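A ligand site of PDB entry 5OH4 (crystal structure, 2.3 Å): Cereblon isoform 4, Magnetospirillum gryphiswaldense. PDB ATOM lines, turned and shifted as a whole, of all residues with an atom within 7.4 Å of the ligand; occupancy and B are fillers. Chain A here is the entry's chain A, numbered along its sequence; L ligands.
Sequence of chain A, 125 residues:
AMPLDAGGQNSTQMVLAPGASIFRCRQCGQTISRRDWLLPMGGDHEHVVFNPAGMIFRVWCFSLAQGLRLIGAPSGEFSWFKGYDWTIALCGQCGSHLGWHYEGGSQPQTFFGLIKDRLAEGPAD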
ATOM      1  N   VAL A  49     -16.235 -32.961   9.537  1.00  0.00           N
ATOM      2  CA  VAL A  49     -17.687 -33.079   9.631  1.00  0.00           C
ATOM      3  C   VAL A  49     -18.320 -33.127   8.249  1.00  0.00           C
ATOM      4  O   VAL A  49     -17.639 -32.864   7.262  1.00  0.00           O
ATOM      5  CB  VAL A  49     -18.278 -31.884  10.385  1.00  0.00           C
ATOM      6  CG1 VAL A  49     -17.821 -31.913  11.826  1.00  0.00           C
ATOM      7  CG2 VAL A  49     -17.855 -30.572   9.739  1.00  0.00           C
ATOM      8  N   PHE A  50     -19.599 -33.529   8.183  1.00  0.00           N
ATOM      9  CA  PHE A  50     -20.393 -33.519   6.930  1.00  0.00           C
ATOM     10  C   PHE A  50     -21.729 -32.828   7.153  1.00  0.00           C
ATOM     11  O   PHE A  50     -22.361 -33.038   8.185  1.00  0.00           O
ATOM     12  CB  PHE A  50     -20.775 -34.914   6.422  1.00  0.00           C
ATOM     13  CG  PHE A  50     -19.633 -35.843   6.285  1.00  0.00           C
ATOM     14  CD1 PHE A  50     -18.846 -35.846   5.124  1.00  0.00           C
ATOM     15  CD2 PHE A  50     -19.336 -36.748   7.290  1.00  0.00           C
ATOM     16  CE1 PHE A  50     -17.782 -36.720   4.982  1.00  0.00           C
ATOM     17  CE2 PHE A  50     -18.272 -37.621   7.149  1.00  0.00           C
ATOM     18  CZ  PHE A  50     -17.497 -37.610   6.003  1.00  0.00           C
ATOM     19  N   ASN A  51     -22.187 -32.120   6.137  1.00  0.00           N
ATOM     20  CA  ASN A  51     -23.555 -31.553   6.097  1.00  0.00           C
ATOM     21  C   ASN A  51     -24.563 -32.496   5.425  1.00  0.00           C
ATOM     22  O   ASN A  51     -24.181 -33.560   4.957  1.00  0.00           O
ATOM     23  CB  ASN A  51     -23.506 -30.151   5.437  1.00  0.00           C
ATOM     24  CG  ASN A  51     -23.310 -30.190   3.931  1.00  0.00           C
ATOM     25  OD1 ASN A  51     -23.433 -31.216   3.279  1.00  0.00           O
ATOM     26  ND2 ASN A  51     -23.073 -29.022   3.372  1.00  0.00           N
ATOM     27  N   PRO A  52     -25.866 -32.153   5.421  1.00  0.00           N
ATOM     28  CA  PRO A  52     -26.847 -33.095   4.839  1.00  0.00           C
ATOM     29  C   PRO A  52     -26.727 -33.322   3.322  1.00  0.00           C
ATOM     30  O   PRO A  52     -27.355 -34.241   2.794  1.00  0.00           O
ATOM     31  CB  PRO A  52     -28.215 -32.468   5.207  1.00  0.00           C
ATOM     32  CG  PRO A  52     -27.938 -31.509   6.318  1.00  0.00           C
ATOM     33  CD  PRO A  52     -26.539 -31.029   6.107  1.00  0.00           C
ATOM     34  N   ALA A  53     -25.959 -32.480   2.627  1.00  0.00           N
ATOM     35  CA  ALA A  53     -25.632 -32.698   1.218  1.00  0.00           C
ATOM     36  C   ALA A  53     -24.349 -33.520   1.019  1.00  0.00           C
ATOM     37  O   ALA A  53     -23.863 -33.688  -0.093  1.00  0.00           O
ATOM     38  CB  ALA A  53     -25.512 -31.356   0.494  1.00  0.00           C
ATOM     39  N   MET A  55     -21.349 -32.977   1.913  1.00  0.00           N
ATOM     40  CA  MET A  55     -20.099 -32.252   1.742  1.00  0.00           C
ATOM     41  C   MET A  55     -19.318 -32.382   3.020  1.00  0.00           C
ATOM     42  O   MET A  55     -19.845 -32.076   4.100  1.00  0.00           O
ATOM     43  CB  MET A  55     -20.303 -30.764   1.421  1.00  0.00           C
ATOM     44  CG  MET A  55     -21.153 -30.503   0.197  1.00  0.00           C
ATOM     45  SD  MET A  55     -21.247 -28.767  -0.290  1.00  0.00           S
ATOM     46  CE  MET A  55     -19.502 -28.319  -0.356  1.00  0.00           C
ATOM     47  N   PHE A  57     -16.247 -31.198   5.299  1.00  0.00           N
ATOM     48  CA  PHE A  57     -15.456 -30.020   5.627  1.00  0.00           C
ATOM     49  C   PHE A  57     -14.506 -30.392   6.711  1.00  0.00           C
ATOM     50  O   PHE A  57     -14.841 -31.107   7.637  1.00  0.00           O
ATOM     51  CB  PHE A  57     -16.330 -28.902   6.157  1.00  0.00           C
ATOM     52  CG  PHE A  57     -17.387 -28.455   5.222  1.00  0.00           C
ATOM     53  CD1 PHE A  57     -17.102 -27.521   4.263  1.00  0.00           C
ATOM     54  CD2 PHE A  57     -18.664 -28.980   5.300  1.00  0.00           C
ATOM     55  CE1 PHE A  57     -18.081 -27.105   3.400  1.00  0.00           C
ATOM     56  CE2 PHE A  57     -19.638 -28.558   4.421  1.00  0.00           C
ATOM     57  CZ  PHE A  57     -19.344 -27.615   3.467  1.00  0.00           C
ATOM     58  N   SER A  75     -29.641 -20.990  13.307  1.00  0.00           N
ATOM     59  CA  SER A  75     -30.444 -22.224  13.235  1.00  0.00           C
ATOM     60  C   SER A  75     -29.742 -23.309  14.061  1.00  0.00           C
ATOM     61  O   SER A  75     -28.523 -23.367  14.112  1.00  0.00           O
ATOM     62  CB  SER A  75     -30.600 -22.673  11.777  1.00  0.00           C
ATOM     63  OG  SER A  75     -31.162 -23.986  11.664  1.00  0.00           O
ATOM     64  N   GLY A  76     -30.516 -24.138  14.714  1.00  0.00           N
ATOM     65  CA  GLY A  76     -29.985 -25.271  15.464  1.00  0.00           C
ATOM     66  C   GLY A  76     -30.001 -26.568  14.673  1.00  0.00           C
ATOM     67  O   GLY A  76     -29.461 -27.579  15.129  1.00  0.00           O
ATOM     68  N   GLU A  77     -30.669 -26.552  13.512  1.00  0.00           N
ATOM     69  CA  GLU A  77     -30.818 -27.733  12.651  1.00  0.00           C
ATOM     70  C   GLU A  77     -29.463 -28.336  12.270  1.00  0.00           C
ATOM     71  O   GLU A  77     -28.611 -27.654  11.687  1.00  0.00           O
ATOM     72  CB  GLU A  77     -31.611 -27.382  11.394  1.00  0.00           C
ATOM     73  CG  GLU A  77     -33.040 -27.933  11.416  1.00  0.00           C
ATOM     74  CD  GLU A  77     -33.725 -27.857  10.058  1.00  0.00           C
ATOM     75  OE1 GLU A  77     -33.480 -26.845   9.323  1.00  0.00           O
ATOM     76  OE2 GLU A  77     -34.480 -28.820   9.717  1.00  0.00           O
ATOM     77  N   PHE A  78     -29.283 -29.593  12.619  1.00  0.00           N
ATOM     78  CA  PHE A  78     -28.102 -30.384  12.234  1.00  0.00           C
ATOM     79  C   PHE A  78     -26.789 -29.793  12.767  1.00  0.00           C
ATOM     80  O   PHE A  78     -25.751 -30.027  12.178  1.00  0.00           O
ATOM     81  CB  PHE A  78     -27.971 -30.535  10.706  1.00  0.00           C
ATOM     82  CG  PHE A  78     -29.218 -31.052  10.008  1.00  0.00           C
ATOM     83  CD1 PHE A  78     -29.640 -32.357  10.184  1.00  0.00           C
ATOM     84  CD2 PHE A  78     -29.899 -30.234   9.094  1.00  0.00           C
ATOM     85  CE1 PHE A  78     -30.758 -32.834   9.523  1.00  0.00           C
ATOM     86  CE2 PHE A  78     -31.021 -30.698   8.437  1.00  0.00           C
ATOM     87  CZ  PHE A  78     -31.455 -32.003   8.648  1.00  0.00           C
ATOM     88  N   SER A  79     -26.822 -29.051  13.867  1.00  0.00           N
ATOM     89  CA  SER A  79     -25.599 -28.447  14.375  1.00  0.00           C
ATOM     90  C   SER A  79     -24.574 -29.510  14.710  1.00  0.00           C
ATOM     91  O   SER A  79     -24.870 -30.480  15.366  1.00  0.00           O
ATOM     92  CB  SER A  79     -25.859 -27.629  15.633  1.00  0.00           C
ATOM     93  OG  SER A  79     -24.656 -26.972  16.030  1.00  0.00           O
ATOM     94  N   TRP A  80     -23.341 -29.303  14.265  1.00  0.00           N
ATOM     95  CA  TRP A  80     -22.247 -30.209  14.584  1.00  0.00           C
ATOM     96  C   TRP A  80     -21.807 -30.106  16.029  1.00  0.00           C
ATOM     97  O   TRP A  80     -21.074 -30.950  16.523  1.00  0.00           O
ATOM     98  CB  TRP A  80     -21.042 -29.919  13.672  1.00  0.00           C
ATOM     99  CG  TRP A  80     -21.281 -30.271  12.244  1.00  0.00           C
ATOM    100  CD1 TRP A  80     -21.821 -31.400  11.776  1.00  0.00           C
ATOM    101  CD2 TRP A  80     -20.979 -29.460  11.112  1.00  0.00           C
ATOM    102  NE1 TRP A  80     -21.889 -31.349  10.399  1.00  0.00           N
ATOM    103  CE2 TRP A  80     -21.372 -30.167   9.975  1.00  0.00           C
ATOM    104  CE3 TRP A  80     -20.400 -28.195  10.960  1.00  0.00           C
ATOM    105  CZ2 TRP A  80     -21.219 -29.659   8.696  1.00  0.00           C
ATOM    106  CZ3 TRP A  80     -20.247 -27.696   9.709  1.00  0.00           C
ATOM    107  CH2 TRP A  80     -20.640 -28.422   8.584  1.00  0.00           C
ATOM    108  N   PHE A  81     -22.200 -29.041  16.718  1.00  0.00           N
ATOM    109  CA  PHE A  81     -21.709 -28.817  18.076  1.00  0.00           C
ATOM    110  C   PHE A  81     -22.883 -28.668  18.993  1.00  0.00           C
ATOM    111  O   PHE A  81     -23.674 -27.710  18.854  1.00  0.00           O
ATOM    112  CB  PHE A  81     -20.820 -27.555  18.137  1.00  0.00           C
ATOM    113  CG  PHE A  81     -19.597 -27.627  17.264  1.00  0.00           C
ATOM    114  CD1 PHE A  81     -18.445 -28.242  17.708  1.00  0.00           C
ATOM    115  CD2 PHE A  81     -19.601 -27.041  16.008  1.00  0.00           C
ATOM    116  CE1 PHE A  81     -17.320 -28.289  16.909  1.00  0.00           C
ATOM    117  CE2 PHE A  81     -18.477 -27.094  15.200  1.00  0.00           C
ATOM    118  CZ  PHE A  81     -17.338 -27.724  15.655  1.00  0.00           C
ATOM    119  N   TYR A  84     -25.288 -25.497  20.291  1.00  0.00           N
ATOM    120  CA  TYR A  84     -25.000 -24.291  19.543  1.00  0.00           C
ATOM    121  C   TYR A  84     -25.883 -24.176  18.316  1.00  0.00           C
ATOM    122  O   TYR A  84     -26.149 -25.186  17.653  1.00  0.00           O
ATOM    123  CB  TYR A  84     -23.526 -24.234  19.112  1.00  0.00           C
ATOM    124  CG  TYR A  84     -22.540 -24.103  20.221  1.00  0.00           C
ATOM    125  CD1 TYR A  84     -22.015 -25.229  20.851  1.00  0.00           C
ATOM    126  CD2 TYR A  84     -22.097 -22.878  20.638  1.00  0.00           C
ATOM    127  CE1 TYR A  84     -21.106 -25.133  21.881  1.00  0.00           C
ATOM    128  CE2 TYR A  84     -21.171 -22.780  21.655  1.00  0.00           C
ATOM    129  CZ  TYR A  84     -20.688 -23.927  22.266  1.00  0.00           C
ATOM    130  OH  TYR A  84     -19.806 -23.846  23.296  1.00  0.00           O
ATOM    131  N   ASP A  85     -26.277 -22.945  17.998  1.00  0.00           N
ATOM    132  CA  ASP A  85     -26.944 -22.588  16.763  1.00  0.00           C
ATOM    133  C   ASP A  85     -25.946 -21.947  15.798  1.00  0.00           C
ATOM    134  O   ASP A  85     -24.981 -21.339  16.229  1.00  0.00           O
ATOM    135  CB  ASP A  85     -28.035 -21.595  17.079  1.00  0.00           C
ATOM    136  CG  ASP A  85     -28.963 -22.112  18.176  1.00  0.00           C
ATOM    137  OD1 ASP A  85     -29.443 -23.273  18.049  1.00  0.00           O
ATOM    138  OD2 ASP A  85     -29.161 -21.376  19.198  1.00  0.00           O
ATOM    139  N   TRP A  86     -26.171 -22.091  14.501  1.00  0.00           N
ATOM    140  CA  TRP A  86     -25.208 -21.651  13.529  1.00  0.00           C
ATOM    141  C   TRP A  86     -25.779 -20.602  12.576  1.00  0.00           C
ATOM    142  O   TRP A  86     -26.986 -20.584  12.256  1.00  0.00           O
ATOM    143  CB  TRP A  86     -24.604 -22.831  12.765  1.00  0.00           C
ATOM    144  CG  TRP A  86     -25.586 -23.750  12.134  1.00  0.00           C
ATOM    145  CD1 TRP A  86     -25.986 -24.948  12.595  1.00  0.00           C
ATOM    146  CD2 TRP A  86     -26.252 -23.570  10.899  1.00  0.00           C
ATOM    147  NE1 TRP A  86     -26.892 -25.512  11.748  1.00  0.00           N
ATOM    148  CE2 TRP A  86     -27.087 -24.678  10.696  1.00  0.00           C
ATOM    149  CE3 TRP A  86     -26.242 -22.560   9.938  1.00  0.00           C
ATOM    150  CZ2 TRP A  86     -27.939 -24.814   9.581  1.00  0.00           C
ATOM    151  CZ3 TRP A  86     -27.077 -22.699   8.799  1.00  0.00           C
ATOM    152  CH2 TRP A  86     -27.916 -23.823   8.641  1.00  0.00           C
ATOM    153  N   THR A  87     -24.904 -19.713  12.113  1.00  0.00           N
ATOM    154  CA  THR A  87     -25.204 -18.844  10.978  1.00  0.00           C
ATOM    155  C   THR A  87     -24.038 -19.011  10.014  1.00  0.00           C
ATOM    156  O   THR A  87     -22.897 -19.155  10.401  1.00  0.00           O
ATOM    157  CB  THR A  87     -25.370 -17.361  11.368  1.00  0.00           C
ATOM    158  OG1 THR A  87     -24.108 -16.891  11.872  1.00  0.00           O
ATOM    159  CG2 THR A  87     -26.333 -17.172  12.444  1.00  0.00           C
ATOM    160  N   ILE A  88     -24.346 -19.013   8.733  1.00  0.00           N
ATOM    161  CA  ILE A  88     -23.355 -19.081   7.688  1.00  0.00           C
ATOM    162  C   ILE A  88     -22.444 -17.839   7.758  1.00  0.00           C
ATOM    163  O   ILE A  88     -22.927 -16.706   7.902  1.00  0.00           O
ATOM    164  CB  ILE A  88     -24.042 -19.174   6.325  1.00  0.00           C
ATOM    165  CG1 ILE A  88     -24.621 -20.590   6.135  1.00  0.00           C
ATOM    166  CG2 ILE A  88     -23.076 -18.878   5.182  1.00  0.00           C
ATOM    167  CD1 ILE A  88     -25.775 -20.652   5.183  1.00  0.00           C
ATOM    168  N   HIS A  97     -17.725 -18.677   0.877  1.00  0.00           N
ATOM    169  CA  HIS A  97     -18.199 -19.314   2.105  1.00  0.00           C
ATOM    170  C   HIS A  97     -17.018 -19.838   2.913  1.00  0.00           C
ATOM    171  O   HIS A  97     -16.318 -20.759   2.500  1.00  0.00           O
ATOM    172  CB  HIS A  97     -19.190 -20.440   1.773  1.00  0.00           C
ATOM    173  CG  HIS A  97     -19.675 -21.192   2.966  1.00  0.00           C
ATOM    174  ND1 HIS A  97     -20.033 -22.522   2.918  1.00  0.00           N
ATOM    175  CD2 HIS A  97     -19.849 -20.811   4.243  1.00  0.00           C
ATOM    176  CE1 HIS A  97     -20.382 -22.928   4.117  1.00  0.00           C
ATOM    177  NE2 HIS A  97     -20.291 -21.909   4.950  1.00  0.00           N
ATOM    178  N   GLY A  99     -17.153 -20.540   6.509  1.00  0.00           N
ATOM    179  CA  GLY A  99     -17.530 -21.342   7.664  1.00  0.00           C
ATOM    180  C   GLY A  99     -18.862 -20.910   8.308  1.00  0.00           C
ATOM    181  O   GLY A  99     -19.845 -20.601   7.625  1.00  0.00           O
ATOM    182  N   TRP A 100     -18.876 -20.936   9.629  1.00  0.00           N
ATOM    183  CA  TRP A 100     -20.103 -20.713  10.390  1.00  0.00           C
ATOM    184  C   TRP A 100     -19.749 -20.005  11.657  1.00  0.00           C
ATOM    185  O   TRP A 100     -18.692 -20.249  12.226  1.00  0.00           O
ATOM    186  CB  TRP A 100     -20.806 -22.059  10.727  1.00  0.00           C
ATOM    187  CG  TRP A 100     -21.223 -22.837   9.530  1.00  0.00           C
ATOM    188  CD1 TRP A 100     -22.425 -22.752   8.867  1.00  0.00           C
ATOM    189  CD2 TRP A 100     -20.396 -23.730   8.764  1.00  0.00           C
ATOM    190  NE1 TRP A 100     -22.387 -23.574   7.756  1.00  0.00           N
ATOM    191  CE2 TRP A 100     -21.165 -24.189   7.694  1.00  0.00           C
ATOM    192  CE3 TRP A 100     -19.087 -24.209   8.907  1.00  0.00           C
ATOM    193  CZ2 TRP A 100     -20.630 -25.086   6.731  1.00  0.00           C
ATOM    194  CZ3 TRP A 100     -18.574 -25.124   7.957  1.00  0.00           C
ATOM    195  CH2 TRP A 100     -19.355 -25.544   6.899  1.00  0.00           C
ATOM    196  N   TYR A 102     -21.023 -19.853  15.527  1.00  0.00           N
ATOM    197  CA  TYR A 102     -21.820 -20.593  16.478  1.00  0.00           C
ATOM    198  C   TYR A 102     -22.106 -19.713  17.689  1.00  0.00           C
ATOM    199  O   TYR A 102     -21.193 -19.024  18.204  1.00  0.00           O
ATOM    200  CB  TYR A 102     -21.099 -21.904  16.854  1.00  0.00           C
ATOM    201  CG  TYR A 102     -21.073 -22.904  15.733  1.00  0.00           C
ATOM    202  CD1 TYR A 102     -22.101 -23.813  15.554  1.00  0.00           C
ATOM    203  CD2 TYR A 102     -19.979 -22.959  14.859  1.00  0.00           C
ATOM    204  CE1 TYR A 102     -22.080 -24.728  14.523  1.00  0.00           C
ATOM    205  CE2 TYR A 102     -19.955 -23.872  13.804  1.00  0.00           C
ATOM    206  CZ  TYR A 102     -21.011 -24.745  13.652  1.00  0.00           C
ATOM    207  OH  TYR A 102     -21.013 -25.654  12.630  1.00  0.00           O
HETATM  208  O1  LIG L   1     -23.191 -27.232  12.210  1.00  0.00           O
HETATM  209  C1  LIG L   1     -23.518 -27.256  11.025  1.00  0.00           C
HETATM  210  N1  LIG L   1     -24.065 -28.345  10.545  1.00  0.00           N
HETATM  211  C2  LIG L   1     -23.273 -26.102  10.066  1.00  0.00           C
HETATM  212  C3  LIG L   1     -24.224 -26.139   8.863  1.00  0.00           C
HETATM  213  C4  LIG L   1     -24.373 -27.520   8.260  1.00  0.00           C
HETATM  214  C5  LIG L   1     -24.400 -28.598   9.298  1.00  0.00           C
HETATM  215  O2  LIG L   1     -24.747 -29.738   9.010  1.00  0.00           O
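OH of Tyr 102 sits at hydrogen-bond distance from O1 of the ligand, at 2.7 Å.
The backbone carbonyl oxygen of Phe 78 is in hydrogen-bond range of a nitrogen (N1) of the ligand (2.9 Å).
An oxygen (O1) of the ligand is in hydrogen-bond range of the backbone NH (N) of Trp 80, 2.9 Å away.
The indole nitrogen (NE1) of Trp 80 is in hydrogen-bond range of the backbone carbonyl oxygen (O) of Phe 50 (2.8 Å).
The backbone carbonyl oxygen (O) of Phe 81 sits at hydrogen-bond distance from the side-chain hydroxyl (OG) of Ser 79.
OG of Ser 79 lies within hydrogen-bond range of O of Tyr 84, 2.8 Å away.
The indole nitrogen (NE1) of Trp 86 lies within hydrogen-bond range of the backbone carbonyl oxygen (O) of Glu 77.
O of Ser 75 is in hydrogen-bond range of N of Trp 86 (2.7 Å).
N of Ala 53 sits at hydrogen-bond distance from OD1 of Asn 51 (2.9 Å).
OD1 of Asn 51 lies within hydrogen-bond range of N of Met 55.
Merely in contact with the ligand: Trp 100 (3.3 Å), Ser 79 (3.5 Å), Trp 86 (3.6 Å), Asn 51 (3.6 Å) and Pro 52 (3.6 Å).
Hydrophobic or aromatic side chains that line the ligand: Pro 52, Phe 78, Trp 80, Trp 86, Trp 100 and Tyr 102.
Of the 23 residues printed, 8 come within 4 Å of the ligand.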
